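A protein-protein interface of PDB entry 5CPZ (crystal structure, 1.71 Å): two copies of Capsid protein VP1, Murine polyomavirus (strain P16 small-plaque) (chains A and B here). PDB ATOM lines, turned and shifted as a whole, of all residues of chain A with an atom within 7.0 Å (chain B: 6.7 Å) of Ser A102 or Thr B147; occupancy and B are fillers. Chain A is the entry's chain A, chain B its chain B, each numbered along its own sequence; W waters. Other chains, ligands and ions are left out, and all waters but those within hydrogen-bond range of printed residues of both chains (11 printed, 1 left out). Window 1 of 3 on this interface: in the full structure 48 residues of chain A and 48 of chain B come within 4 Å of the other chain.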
ATOM      1  N   GLN A  39      42.355  21.875 -31.670  1.00  0.00           N
ATOM      2  CA  GLN A  39      41.032  21.334 -31.997  1.00  0.00           C
ATOM      3  C   GLN A  39      40.579  20.253 -31.006  1.00  0.00           C
ATOM      4  O   GLN A  39      39.388  19.960 -30.916  1.00  0.00           O
ATOM      5  CB  GLN A  39      40.971  20.812 -33.447  1.00  0.00           C
ATOM      6  CG  GLN A  39      41.828  19.583 -33.751  1.00  0.00           C
ATOM      7  CD  GLN A  39      43.218  19.920 -34.270  1.00  0.00           C
ATOM      8  OE1 GLN A  39      43.893  20.816 -33.755  1.00  0.00           O
ATOM      9  NE2 GLN A  39      43.660  19.191 -35.296  1.00  0.00           N
ATOM     10  N   TYR A  41      41.083  20.539 -27.666  1.00  0.00           N
ATOM     11  CA  TYR A  41      40.914  21.125 -26.337  1.00  0.00           C
ATOM     12  C   TYR A  41      39.460  20.981 -25.856  1.00  0.00           C
ATOM     13  O   TYR A  41      38.521  21.332 -26.571  1.00  0.00           O
ATOM     14  CB  TYR A  41      41.413  22.587 -26.303  1.00  0.00           C
ATOM     15  CG  TYR A  41      41.380  23.229 -24.928  1.00  0.00           C
ATOM     16  CD1 TYR A  41      41.716  22.499 -23.780  1.00  0.00           C
ATOM     17  CD2 TYR A  41      41.045  24.575 -24.778  1.00  0.00           C
ATOM     18  CE1 TYR A  41      41.681  23.090 -22.520  1.00  0.00           C
ATOM     19  CE2 TYR A  41      41.021  25.177 -23.528  1.00  0.00           C
ATOM     20  CZ  TYR A  41      41.341  24.435 -22.402  1.00  0.00           C
ATOM     21  OH  TYR A  41      41.308  25.042 -21.159  1.00  0.00           O
ATOM     22  N   TRP A  43      38.753  17.871 -24.912  1.00  0.00           N
ATOM     23  CA  TRP A  43      38.708  16.439 -25.206  1.00  0.00           C
ATOM     24  C   TRP A  43      40.040  15.791 -24.847  1.00  0.00           C
ATOM     25  O   TRP A  43      41.038  16.480 -24.636  1.00  0.00           O
ATOM     26  CB  TRP A  43      38.453  16.197 -26.705  1.00  0.00           C
ATOM     27  CG  TRP A  43      37.291  16.967 -27.282  1.00  0.00           C
ATOM     28  CD1 TRP A  43      37.296  18.275 -27.684  1.00  0.00           C
ATOM     29  CD2 TRP A  43      35.973  16.470 -27.549  1.00  0.00           C
ATOM     30  NE1 TRP A  43      36.056  18.631 -28.158  1.00  0.00           N
ATOM     31  CE2 TRP A  43      35.223  17.544 -28.091  1.00  0.00           C
ATOM     32  CE3 TRP A  43      35.347  15.224 -27.377  1.00  0.00           C
ATOM     33  CZ2 TRP A  43      33.879  17.412 -28.466  1.00  0.00           C
ATOM     34  CZ3 TRP A  43      34.005  15.098 -27.741  1.00  0.00           C
ATOM     35  CH2 TRP A  43      33.290  16.185 -28.285  1.00  0.00           C
ATOM     36  N   VAL A  98      28.381  23.381 -17.277  1.00  0.00           N
ATOM     37  CA  VAL A  98      27.876  24.200 -18.384  1.00  0.00           C
ATOM     38  C   VAL A  98      28.195  23.561 -19.729  1.00  0.00           C
ATOM     39  O   VAL A  98      29.291  23.028 -19.926  1.00  0.00           O
ATOM     40  CB  VAL A  98      28.483  25.625 -18.347  1.00  0.00           C
ATOM     41  CG1 VAL A  98      27.941  26.501 -19.480  1.00  0.00           C
ATOM     42  CG2 VAL A  98      28.193  26.279 -17.007  1.00  0.00           C
ATOM     43  N   GLY A  99      27.226  23.612 -20.640  1.00  0.00           N
ATOM     44  CA  GLY A  99      27.469  23.246 -22.031  1.00  0.00           C
ATOM     45  C   GLY A  99      26.927  21.910 -22.502  1.00  0.00           C
ATOM     46  O   GLY A  99      27.293  21.463 -23.588  1.00  0.00           O
ATOM     47  N   SER A 100      26.050  21.266 -21.721  1.00  0.00           N
ATOM     48  CA  SER A 100      25.473  19.987 -22.187  1.00  0.00           C
ATOM     49  C   SER A 100      24.751  20.130 -23.534  1.00  0.00           C
ATOM     50  O   SER A 100      24.763  19.207 -24.348  1.00  0.00           O
ATOM     51  CB  SER A 100      24.564  19.319 -21.140  1.00  0.00           C
ATOM     52  OG  SER A 100      23.468  20.142 -20.786  1.00  0.00           O
ATOM     53  N   GLY A 101      24.135  21.290 -23.772  1.00  0.00           N
ATOM     54  CA  GLY A 101      23.494  21.570 -25.062  1.00  0.00           C
ATOM     55  C   GLY A 101      24.398  21.374 -26.273  1.00  0.00           C
ATOM     56  O   GLY A 101      23.913  21.046 -27.355  1.00  0.00           O
ATOM     57  N   SER A 102      25.706  21.557 -26.097  1.00  0.00           N
ATOM     58  CA  SER A 102      26.671  21.366 -27.189  1.00  0.00           C
ATOM     59  C   SER A 102      26.735  19.909 -27.666  1.00  0.00           C
ATOM     60  O   SER A 102      27.166  19.634 -28.786  1.00  0.00           O
ATOM     61  CB  SER A 102      28.069  21.847 -26.784  1.00  0.00           C
ATOM     62  OG  SER A 102      28.684  20.961 -25.858  1.00  0.00           O
ATOM     63  N   LEU A 103      26.291  18.978 -26.822  1.00  0.00           N
ATOM     64  CA  LEU A 103      26.271  17.562 -27.201  1.00  0.00           C
ATOM     65  C   LEU A 103      25.154  17.254 -28.208  1.00  0.00           C
ATOM     66  O   LEU A 103      25.093  16.152 -28.762  1.00  0.00           O
ATOM     67  CB  LEU A 103      26.175  16.663 -25.958  1.00  0.00           C
ATOM     68  CG  LEU A 103      27.242  16.877 -24.876  1.00  0.00           C
ATOM     69  CD1 LEU A 103      26.953  15.973 -23.686  1.00  0.00           C
ATOM     70  CD2 LEU A 103      28.645  16.636 -25.414  1.00  0.00           C
ATOM     71  N   LEU A 104      24.283  18.235 -28.444  1.00  0.00           N
ATOM     72  CA  LEU A 104      23.234  18.122 -29.461  1.00  0.00           C
ATOM     73  C   LEU A 104      23.770  18.357 -30.880  1.00  0.00           C
ATOM     74  O   LEU A 104      23.008  18.312 -31.847  1.00  0.00           O
ATOM     75  CB  LEU A 104      22.088  19.100 -29.176  1.00  0.00           C
ATOM     76  CG  LEU A 104      21.365  18.939 -27.829  1.00  0.00           C
ATOM     77  CD1 LEU A 104      20.526  20.177 -27.553  1.00  0.00           C
ATOM     78  CD2 LEU A 104      20.486  17.694 -27.826  1.00  0.00           C
ATOM     79  N   ASP A 105      25.068  18.623 -30.994  1.00  0.00           N
ATOM     80  CA  ASP A 105      25.724  18.650 -32.305  1.00  0.00           C
ATOM     81  C   ASP A 105      25.899  17.212 -32.798  1.00  0.00           C
ATOM     82  O   ASP A 105      26.825  16.511 -32.385  1.00  0.00           O
ATOM     83  CB  ASP A 105      27.074  19.384 -32.225  1.00  0.00           C
ATOM     84  CG  ASP A 105      27.913  19.244 -33.502  1.00  0.00           C
ATOM     85  OD1 ASP A 105      27.473  18.596 -34.475  1.00  0.00           O
ATOM     86  OD2 ASP A 105      29.038  19.788 -33.528  1.00  0.00           O
ATOM     87  N   VAL A 106      24.982  16.776 -33.661  1.00  0.00           N
ATOM     88  CA  VAL A 106      25.059  15.455 -34.290  1.00  0.00           C
ATOM     89  C   VAL A 106      25.264  15.599 -35.807  1.00  0.00           C
ATOM     90  O   VAL A 106      24.884  14.724 -36.595  1.00  0.00           O
ATOM     91  CB  VAL A 106      23.835  14.559 -33.948  1.00  0.00           C
ATOM     92  CG1 VAL A 106      23.799  14.271 -32.446  1.00  0.00           C
ATOM     93  CG2 VAL A 106      22.523  15.182 -34.423  1.00  0.00           C
ATOM     94  N   HIS A 107      25.887  16.709 -36.205  1.00  0.00           N
ATOM     95  CA  HIS A 107      26.115  16.988 -37.627  1.00  0.00           C
ATOM     96  C   HIS A 107      27.594  16.924 -38.019  1.00  0.00           C
ATOM     97  O   HIS A 107      27.947  17.255 -39.153  1.00  0.00           O
ATOM     98  CB  HIS A 107      25.515  18.351 -38.019  1.00  0.00           C
ATOM     99  CG  HIS A 107      26.054  19.499 -37.226  1.00  0.00           C
ATOM    100  ND1 HIS A 107      27.317  20.017 -37.428  1.00  0.00           N
ATOM    101  CD2 HIS A 107      25.502  20.230 -36.227  1.00  0.00           C
ATOM    102  CE1 HIS A 107      27.524  21.011 -36.582  1.00  0.00           C
ATOM    103  NE2 HIS A 107      26.437  21.162 -35.842  1.00  0.00           N
ATOM    104  N   GLY A 108      28.447  16.498 -37.086  1.00  0.00           N
ATOM    105  CA  GLY A 108      29.895  16.393 -37.332  1.00  0.00           C
ATOM    106  C   GLY A 108      30.338  15.153 -38.092  1.00  0.00           C
ATOM    107  O   GLY A 108      29.540  14.516 -38.788  1.00  0.00           O
ATOM    108  N   ASN A 110      31.822  12.336 -36.731  1.00  0.00           N
ATOM    109  CA  ASN A 110      31.973  11.135 -35.897  1.00  0.00           C
ATOM    110  C   ASN A 110      31.505   9.899 -36.656  1.00  0.00           C
ATOM    111  O   ASN A 110      30.889  10.011 -37.715  1.00  0.00           O
ATOM    112  CB  ASN A 110      31.157  11.239 -34.599  1.00  0.00           C
ATOM    113  CG  ASN A 110      31.553  12.419 -33.725  1.00  0.00           C
ATOM    114  OD1 ASN A 110      32.611  13.031 -33.903  1.00  0.00           O
ATOM    115  ND2 ASN A 110      30.697  12.736 -32.755  1.00  0.00           N
ATOM    116  N   VAL A 125      28.165  12.060 -28.168  1.00  0.00           N
ATOM    117  CA  VAL A 125      28.960  11.600 -27.023  1.00  0.00           C
ATOM    118  C   VAL A 125      28.115  10.645 -26.166  1.00  0.00           C
ATOM    119  O   VAL A 125      26.966  10.946 -25.869  1.00  0.00           O
ATOM    120  CB  VAL A 125      29.453  12.800 -26.188  1.00  0.00           C
ATOM    121  CG1 VAL A 125      30.001  12.346 -24.835  1.00  0.00           C
ATOM    122  CG2 VAL A 125      30.513  13.573 -26.970  1.00  0.00           C
ATOM    123  N   ARG A 257      33.417  10.641 -27.708  1.00  0.00           N
ATOM    124  CA  ARG A 257      33.035  10.597 -29.118  1.00  0.00           C
ATOM    125  C   ARG A 257      33.895   9.527 -29.790  1.00  0.00           C
ATOM    126  O   ARG A 257      34.989   9.197 -29.302  1.00  0.00           O
ATOM    127  CB  ARG A 257      33.180  11.962 -29.810  1.00  0.00           C
ATOM    128  CG  ARG A 257      34.611  12.387 -30.095  1.00  0.00           C
ATOM    129  CD  ARG A 257      34.659  13.682 -30.892  1.00  0.00           C
ATOM    130  NE  ARG A 257      36.036  14.109 -31.107  1.00  0.00           N
ATOM    131  CZ  ARG A 257      36.796  13.699 -32.116  1.00  0.00           C
ATOM    132  NH1 ARG A 257      36.309  12.856 -33.017  1.00  0.00           N
ATOM    133  NH2 ARG A 257      38.041  14.138 -32.232  1.00  0.00           N
ATOM    134  N   ARG A 268      35.185  13.357 -23.552  1.00  0.00           N
ATOM    135  CA  ARG A 268      34.654  14.726 -23.546  1.00  0.00           C
ATOM    136  C   ARG A 268      34.394  15.173 -22.115  1.00  0.00           C
ATOM    137  O   ARG A 268      33.746  14.456 -21.345  1.00  0.00           O
ATOM    138  CB  ARG A 268      33.338  14.819 -24.341  1.00  0.00           C
ATOM    139  CG  ARG A 268      32.659  16.199 -24.345  1.00  0.00           C
ATOM    140  CD  ARG A 268      33.603  17.326 -24.766  1.00  0.00           C
ATOM    141  NE  ARG A 268      32.929  18.491 -25.356  1.00  0.00           N
ATOM    142  CZ  ARG A 268      33.396  19.739 -25.305  1.00  0.00           C
ATOM    143  NH1 ARG A 268      34.519  20.007 -24.639  1.00  0.00           N
ATOM    144  NH2 ARG A 268      32.739  20.729 -25.908  1.00  0.00           N
ATOM    145  N   LEU A 270      33.315  18.802 -19.603  1.00  0.00           N
ATOM    146  CA  LEU A 270      32.678  20.113 -19.628  1.00  0.00           C
ATOM    147  C   LEU A 270      33.120  20.948 -18.433  1.00  0.00           C
ATOM    148  O   LEU A 270      33.460  20.393 -17.392  1.00  0.00           O
ATOM    149  CB  LEU A 270      31.147  19.982 -19.651  1.00  0.00           C
ATOM    150  CG  LEU A 270      30.500  19.488 -20.953  1.00  0.00           C
ATOM    151  CD1 LEU A 270      29.003  19.303 -20.745  1.00  0.00           C
ATOM    152  CD2 LEU A 270      30.763  20.435 -22.128  1.00  0.00           C
ATOM    153  N   ASP B  56      32.606  21.074 -41.750  1.00  0.00           N
ATOM    154  CA  ASP B  56      31.339  20.892 -41.057  1.00  0.00           C
ATOM    155  C   ASP B  56      30.485  22.149 -41.233  1.00  0.00           C
ATOM    156  O   ASP B  56      30.702  23.152 -40.544  1.00  0.00           O
ATOM    157  CB  ASP B  56      31.605  20.608 -39.567  1.00  0.00           C
ATOM    158  CG  ASP B  56      30.335  20.422 -38.757  1.00  0.00           C
ATOM    159  OD1 ASP B  56      29.303  19.992 -39.318  1.00  0.00           O
ATOM    160  OD2 ASP B  56      30.378  20.698 -37.536  1.00  0.00           O
ATOM    161  N   TYR B 130      16.288  17.535 -24.723  1.00  0.00           N
ATOM    162  CA  TYR B 130      16.817  18.736 -24.100  1.00  0.00           C
ATOM    163  C   TYR B 130      15.652  19.627 -23.705  1.00  0.00           C
ATOM    164  O   TYR B 130      14.861  20.031 -24.552  1.00  0.00           O
ATOM    165  CB  TYR B 130      17.733  19.453 -25.095  1.00  0.00           C
ATOM    166  CG  TYR B 130      18.568  20.588 -24.535  1.00  0.00           C
ATOM    167  CD1 TYR B 130      19.511  20.372 -23.520  1.00  0.00           C
ATOM    168  CD2 TYR B 130      18.443  21.877 -25.057  1.00  0.00           C
ATOM    169  CE1 TYR B 130      20.290  21.418 -23.031  1.00  0.00           C
ATOM    170  CE2 TYR B 130      19.216  22.922 -24.577  1.00  0.00           C
ATOM    171  CZ  TYR B 130      20.136  22.692 -23.571  1.00  0.00           C
ATOM    172  OH  TYR B 130      20.901  23.745 -23.117  1.00  0.00           O
ATOM    173  N   LEU B 145      29.412  27.812 -25.963  1.00  0.00           N
ATOM    174  CA  LEU B 145      30.305  26.655 -25.838  1.00  0.00           C
ATOM    175  C   LEU B 145      29.898  25.669 -26.919  1.00  0.00           C
ATOM    176  O   LEU B 145      28.723  25.293 -27.009  1.00  0.00           O
ATOM    177  CB  LEU B 145      30.209  25.991 -24.451  1.00  0.00           C
ATOM    178  CG  LEU B 145      31.216  24.870 -24.134  1.00  0.00           C
ATOM    179  CD1 LEU B 145      31.440  24.747 -22.632  1.00  0.00           C
ATOM    180  CD2 LEU B 145      30.794  23.510 -24.693  1.00  0.00           C
ATOM    181  N   VAL B 146      30.865  25.256 -27.736  1.00  0.00           N
ATOM    182  CA  VAL B 146      30.574  24.386 -28.880  1.00  0.00           C
ATOM    183  C   VAL B 146      31.334  23.060 -28.827  1.00  0.00           C
ATOM    184  O   VAL B 146      32.357  22.931 -28.151  1.00  0.00           O
ATOM    185  CB  VAL B 146      30.853  25.092 -30.237  1.00  0.00           C
ATOM    186  CG1 VAL B 146      29.991  26.344 -30.374  1.00  0.00           C
ATOM    187  CG2 VAL B 146      32.330  25.442 -30.384  1.00  0.00           C
ATOM    188  N   THR B 147      30.824  22.081 -29.566  1.00  0.00           N
ATOM    189  CA  THR B 147      31.545  20.842 -29.826  1.00  0.00           C
ATOM    190  C   THR B 147      32.853  21.096 -30.587  1.00  0.00           C
ATOM    191  O   THR B 147      33.920  20.575 -30.219  1.00  0.00           O
ATOM    192  CB  THR B 147      30.633  19.848 -30.586  1.00  0.00           C
ATOM    193  OG1 THR B 147      29.703  19.273 -29.660  1.00  0.00           O
ATOM    194  CG2 THR B 147      31.440  18.723 -31.248  1.00  0.00           C
ATOM    195  N   ASP B 148      32.775  21.921 -31.631  1.00  0.00           N
ATOM    196  CA  ASP B 148      33.885  22.097 -32.550  1.00  0.00           C
ATOM    197  C   ASP B 148      33.975  23.560 -32.975  1.00  0.00           C
ATOM    198  O   ASP B 148      33.080  24.079 -33.644  1.00  0.00           O
ATOM    199  CB  ASP B 148      33.695  21.178 -33.768  1.00  0.00           C
ATOM    200  CG  ASP B 148      34.945  21.065 -34.635  1.00  0.00           C
ATOM    201  OD1 ASP B 148      35.865  21.899 -34.509  1.00  0.00           O
ATOM    202  OD2 ASP B 148      35.003  20.122 -35.450  1.00  0.00           O
ATOM    203  N   ALA B 149      35.060  24.218 -32.569  1.00  0.00           N
ATOM    204  CA  ALA B 149      35.304  25.621 -32.904  1.00  0.00           C
ATOM    205  C   ALA B 149      35.540  25.811 -34.407  1.00  0.00           C
ATOM    206  O   ALA B 149      35.561  26.943 -34.901  1.00  0.00           O
ATOM    207  CB  ALA B 149      36.493  26.154 -32.112  1.00  0.00           C
ATOM    208  N   ARG B 150      35.724  24.700 -35.117  1.00  0.00           N
ATOM    209  CA  ARG B 150      35.943  24.726 -36.561  1.00  0.00           C
ATOM    210  C   ARG B 150      34.638  24.659 -37.351  1.00  0.00           C
ATOM    211  O   ARG B 150      34.658  24.817 -38.579  1.00  0.00           O
ATOM    212  CB  ARG B 150      36.861  23.581 -36.990  1.00  0.00           C
ATOM    213  CG  ARG B 150      38.230  23.591 -36.321  1.00  0.00           C
ATOM    214  CD  ARG B 150      38.977  22.299 -36.596  1.00  0.00           C
ATOM    215  NE  ARG B 150      38.194  21.138 -36.172  1.00  0.00           N
ATOM    216  CZ  ARG B 150      38.503  19.876 -36.451  1.00  0.00           C
ATOM    217  NH1 ARG B 150      39.596  19.593 -37.154  1.00  0.00           N
ATOM    218  NH2 ARG B 150      37.707  18.894 -36.026  1.00  0.00           N
ATOM    219  N   THR B 151      33.522  24.423 -36.664  1.00  0.00           N
ATOM    220  CA  THR B 151      32.213  24.338 -37.328  1.00  0.00           C
ATOM    221  C   THR B 151      31.926  25.634 -38.085  1.00  0.00           C
ATOM    222  O   THR B 151      32.060  26.727 -37.531  1.00  0.00           O
ATOM    223  CB  THR B 151      31.069  24.038 -36.343  1.00  0.00           C
ATOM    224  OG1 THR B 151      31.257  22.728 -35.785  1.00  0.00           O
ATOM    225  CG2 THR B 151      29.709  24.093 -37.056  1.00  0.00           C
ATOM    226  N   TYR B 153      29.354  27.622 -39.189  1.00  0.00           N
ATOM    227  CA  TYR B 153      27.976  28.105 -39.115  1.00  0.00           C
ATOM    228  C   TYR B 153      27.763  29.196 -40.158  1.00  0.00           C
ATOM    229  O   TYR B 153      28.689  29.955 -40.458  1.00  0.00           O
ATOM    230  CB  TYR B 153      27.663  28.657 -37.719  1.00  0.00           C
ATOM    231  CG  TYR B 153      27.696  27.612 -36.625  1.00  0.00           C
ATOM    232  CD1 TYR B 153      26.693  26.646 -36.527  1.00  0.00           C
ATOM    233  CD2 TYR B 153      28.729  27.593 -35.684  1.00  0.00           C
ATOM    234  CE1 TYR B 153      26.717  25.687 -35.526  1.00  0.00           C
ATOM    235  CE2 TYR B 153      28.763  26.638 -34.677  1.00  0.00           C
ATOM    236  CZ  TYR B 153      27.759  25.686 -34.609  1.00  0.00           C
ATOM    237  OH  TYR B 153      27.791  24.739 -33.611  1.00  0.00           O
ATOM    238  N   ASP B 173      36.658  28.122 -27.122  1.00  0.00           N
ATOM    239  CA  ASP B 173      35.198  28.051 -27.287  1.00  0.00           C
ATOM    240  C   ASP B 173      34.622  26.636 -27.171  1.00  0.00           C
ATOM    241  O   ASP B 173      33.400  26.466 -27.094  1.00  0.00           O
ATOM    242  CB  ASP B 173      34.768  28.714 -28.605  1.00  0.00           C
ATOM    243  CG  ASP B 173      34.976  30.223 -28.592  1.00  0.00           C
ATOM    244  OD1 ASP B 173      34.822  30.842 -27.515  1.00  0.00           O
ATOM    245  OD2 ASP B 173      35.296  30.787 -29.659  1.00  0.00           O
ATOM    246  N   GLN B 174      35.501  25.630 -27.142  1.00  0.00           N
ATOM    247  CA  GLN B 174      35.104  24.237 -26.882  1.00  0.00           C
ATOM    248  C   GLN B 174      35.049  23.936 -25.382  1.00  0.00           C
ATOM    249  O   GLN B 174      34.573  22.877 -24.966  1.00  0.00           O
ATOM    250  CB  GLN B 174      36.041  23.262 -27.605  1.00  0.00           C
ATOM    251  CG  GLN B 174      35.956  23.424 -29.118  1.00  0.00           C
ATOM    252  CD  GLN B 174      36.906  22.542 -29.912  1.00  0.00           C
ATOM    253  OE1 GLN B 174      36.977  22.663 -31.138  1.00  0.00           O
ATOM    254  NE2 GLN B 174      37.639  21.658 -29.234  1.00  0.00           N
ATOM    255  N   VAL B 192      20.826  26.105 -29.863  1.00  0.00           N
ATOM    256  CA  VAL B 192      20.992  25.512 -28.534  1.00  0.00           C
ATOM    257  C   VAL B 192      22.268  24.666 -28.425  1.00  0.00           C
ATOM    258  O   VAL B 192      22.744  24.397 -27.322  1.00  0.00           O
ATOM    259  CB  VAL B 192      19.728  24.750 -28.073  1.00  0.00           C
ATOM    260  CG1 VAL B 192      18.545  25.712 -27.994  1.00  0.00           C
ATOM    261  CG2 VAL B 192      19.405  23.580 -29.000  1.00  0.00           C
ATOM    262  N   GLU B 193      22.839  24.271 -29.561  1.00  0.00           N
ATOM    263  CA  GLU B 193      24.128  23.579 -29.528  1.00  0.00           C
ATOM    264  C   GLU B 193      25.306  24.547 -29.321  1.00  0.00           C
ATOM    265  O   GLU B 193      26.451  24.112 -29.162  1.00  0.00           O
ATOM    266  CB  GLU B 193      24.330  22.700 -30.770  1.00  0.00           C
ATOM    267  CG  GLU B 193      24.698  23.456 -32.040  1.00  0.00           C
ATOM    268  CD  GLU B 193      25.118  22.518 -33.155  1.00  0.00           C
ATOM    269  OE1 GLU B 193      24.473  21.465 -33.322  1.00  0.00           O
ATOM    270  OE2 GLU B 193      26.093  22.836 -33.864  1.00  0.00           O
ATOM    271  N   ILE B 194      25.012  25.850 -29.308  1.00  0.00           N
ATOM    272  CA  ILE B 194      26.036  26.884 -29.098  1.00  0.00           C
ATOM    273  C   ILE B 194      25.818  27.650 -27.789  1.00  0.00           C
ATOM    274  O   ILE B 194      26.771  27.908 -27.060  1.00  0.00           O
ATOM    275  CB  ILE B 194      26.066  27.917 -30.249  1.00  0.00           C
ATOM    276  CG1 ILE B 194      26.377  27.242 -31.593  1.00  0.00           C
ATOM    277  CG2 ILE B 194      27.075  29.036 -29.962  1.00  0.00           C
ATOM    278  CD1 ILE B 194      26.122  28.147 -32.789  1.00  0.00           C
ATOM    279  N   HIS B 196      24.217  28.573 -24.092  1.00  0.00           N
ATOM    280  CA  HIS B 196      23.775  27.955 -22.840  1.00  0.00           C
ATOM    281  C   HIS B 196      23.473  29.023 -21.810  1.00  0.00           C
ATOM    282  O   HIS B 196      24.037  30.118 -21.886  1.00  0.00           O
ATOM    283  CB  HIS B 196      24.897  27.045 -22.339  1.00  0.00           C
ATOM    284  CG  HIS B 196      25.511  26.257 -23.447  1.00  0.00           C
ATOM    285  ND1 HIS B 196      24.885  25.163 -24.002  1.00  0.00           N
ATOM    286  CD2 HIS B 196      26.626  26.474 -24.187  1.00  0.00           C
ATOM    287  CE1 HIS B 196      25.610  24.712 -25.011  1.00  0.00           C
ATOM    288  NE2 HIS B 196      26.667  25.495 -25.150  1.00  0.00           N
ATOM    289  N   TYR B 211      19.266  17.454 -19.789  1.00  0.00           N
ATOM    290  CA  TYR B 211      19.746  16.861 -21.025  1.00  0.00           C
ATOM    291  C   TYR B 211      19.817  15.358 -20.836  1.00  0.00           C
ATOM    292  O   TYR B 211      20.316  14.880 -19.814  1.00  0.00           O
ATOM    293  CB  TYR B 211      21.150  17.395 -21.361  1.00  0.00           C
ATOM    294  CG  TYR B 211      21.835  16.621 -22.475  1.00  0.00           C
ATOM    295  CD1 TYR B 211      21.530  16.879 -23.810  1.00  0.00           C
ATOM    296  CD2 TYR B 211      22.769  15.620 -22.191  1.00  0.00           C
ATOM    297  CE1 TYR B 211      22.135  16.168 -24.836  1.00  0.00           C
ATOM    298  CE2 TYR B 211      23.378  14.898 -23.216  1.00  0.00           C
ATOM    299  CZ  TYR B 211      23.056  15.178 -24.532  1.00  0.00           C
ATOM    300  OH  TYR B 211      23.638  14.483 -25.567  1.00  0.00           O
HETATM  301  O   HOH W   1      22.817  14.882 -28.070  1.00  0.00           O
HETATM  302  O   HOH W   2      28.795  16.661 -30.362  1.00  0.00           O
HETATM  303  O   HOH W   3      38.506  17.370 -33.015  1.00  0.00           O
HETATM  304  O   HOH W   4      35.428  18.721 -31.519  1.00  0.00           O
HETATM  305  O   HOH W   5      21.848  21.020 -32.827  1.00  0.00           O
HETATM  306  O   HOH W   6      24.451  11.824 -26.439  1.00  0.00           O
HETATM  307  O   HOH W   7      27.136  19.653 -41.215  1.00  0.00           O
HETATM  308  O   HOH W   8      30.226  22.486 -33.079  1.00  0.00           O
HETATM  309  O   HOH W   9      30.636  19.013 -35.480  1.00  0.00           O
HETATM  310  O   HOH W  10      30.474  19.157 -26.931  1.00  0.00           O
HETATM  311  O   HOH W  11      23.437  23.627 -22.171  1.00  0.00           O
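The backbone carbonyl oxygen (O) of Gln A39 is in hydrogen-bond range of the side-chain amide nitrogen (NE2) of Gln B174.
The backbone carbonyl oxygen (O) of Tyr A41 sits at hydrogen-bond distance from the side-chain amide nitrogen (NE2) of Gln B174, at 2.8 Å.
The backbone carbonyl oxygen of Ser A102 is in hydrogen-bond range of the side-chain hydroxyl of Thr B147 (2.7 Å).
A ring nitrogen (ND1) of His A107 lies within hydrogen-bond range of the side-chain carboxylate of Asp B56, at 2.7 Å.
A ring nitrogen (NE2) of His A107 sits at hydrogen-bond distance from the side-chain carboxylate of Glu B193, 2.6 Å away.
The guanidinium group of Arg A268 is in hydrogen-bond range of the backbone carbonyl oxygen of Val B146, at 3.2 Å.
The guanidinium group (NH1) of Arg A268 lies within hydrogen-bond range of the backbone carbonyl oxygen (O) of Gln B174 (2.9 Å).
The backbone carbonyl oxygen (O) of Gly A99 sits at hydrogen-bond distance from the side-chain hydroxyl (OG) of Ser A102.
The backbone NH (N) of Gly A108 is in hydrogen-bond range of the side-chain carboxylate (OD1) of Asp A105.
O of Ile B194 sits at hydrogen-bond distance from N of Leu B145 (2.9 Å).
Gln A39 touches Arg B150 (CB to NE, 3.9 Å).
Gly A99 touches His B196 (CA to ND1, 3.8 Å).
Tyr B211 touches Ser A100.
O of Gly A101 touches CA of Glu B193 (3.3 Å).
Gly A101 touches His B196 (C to CE1, 3.8 Å).
Ser A102 touches Glu B193 (CA to O, 3.4 Å).
Leu A104 touches Tyr B130 (CD1 to CG, 3.6 Å).
Arg A268 touches Leu B145 (NH2 to CD2, 3.6 Å).
Of the printed residues of chain B, Ser A102 touches Leu B145 (3.5 Å), Thr B147 (2.7 Å), Glu B193 (3.4 Å) and His B196 (3.3 Å).
Thr B147 touches just these residues of chain A: Trp A43 (3.5 Å), Ser A102 (2.7 Å) and Asp A105 (3.3 Å).
Of the printed residues of chain A, His B196 touches Gly A99, Gly A101 and Ser A102.
Printed residues of chain B within 4 Å of Val A98: Leu B145.
Leu A270 touches none of the printed residues of chain B.
The nearest residue of chain B that does not touch Ser A102 is Val B146 (4.04 Å).
The nearest printed residue of chain B that does not touch Leu A103 is Thr B147 (4.4 Å).
Of the 19 printed residues of chain A, 13 touch a printed residue of chain B.
Hydrophobic or aromatic side chains of chain B within 4 Å of the printed part of chain A: Tyr B130, Leu B145, Val B192, His B196 and Tyr B211.
Among the printed residues, no Asp or Glu carboxylate lies within 4 Å of a Lys or Arg side-chain nitrogen of the other chain.
No position is printed for both chains.
Of the 29 pairs that touch across the chains among the printed residues, none has its exchanged pair printed and touching as well.
Water W3 lies within hydrogen-bond range of the guanidinium group (NH2) of Arg A257 (3.4 Å), the backbone carbonyl oxygen (O) of Gln A39 (3.4 Å) and the guanidinium group (NH2) of Arg B150 (3.5 Å).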
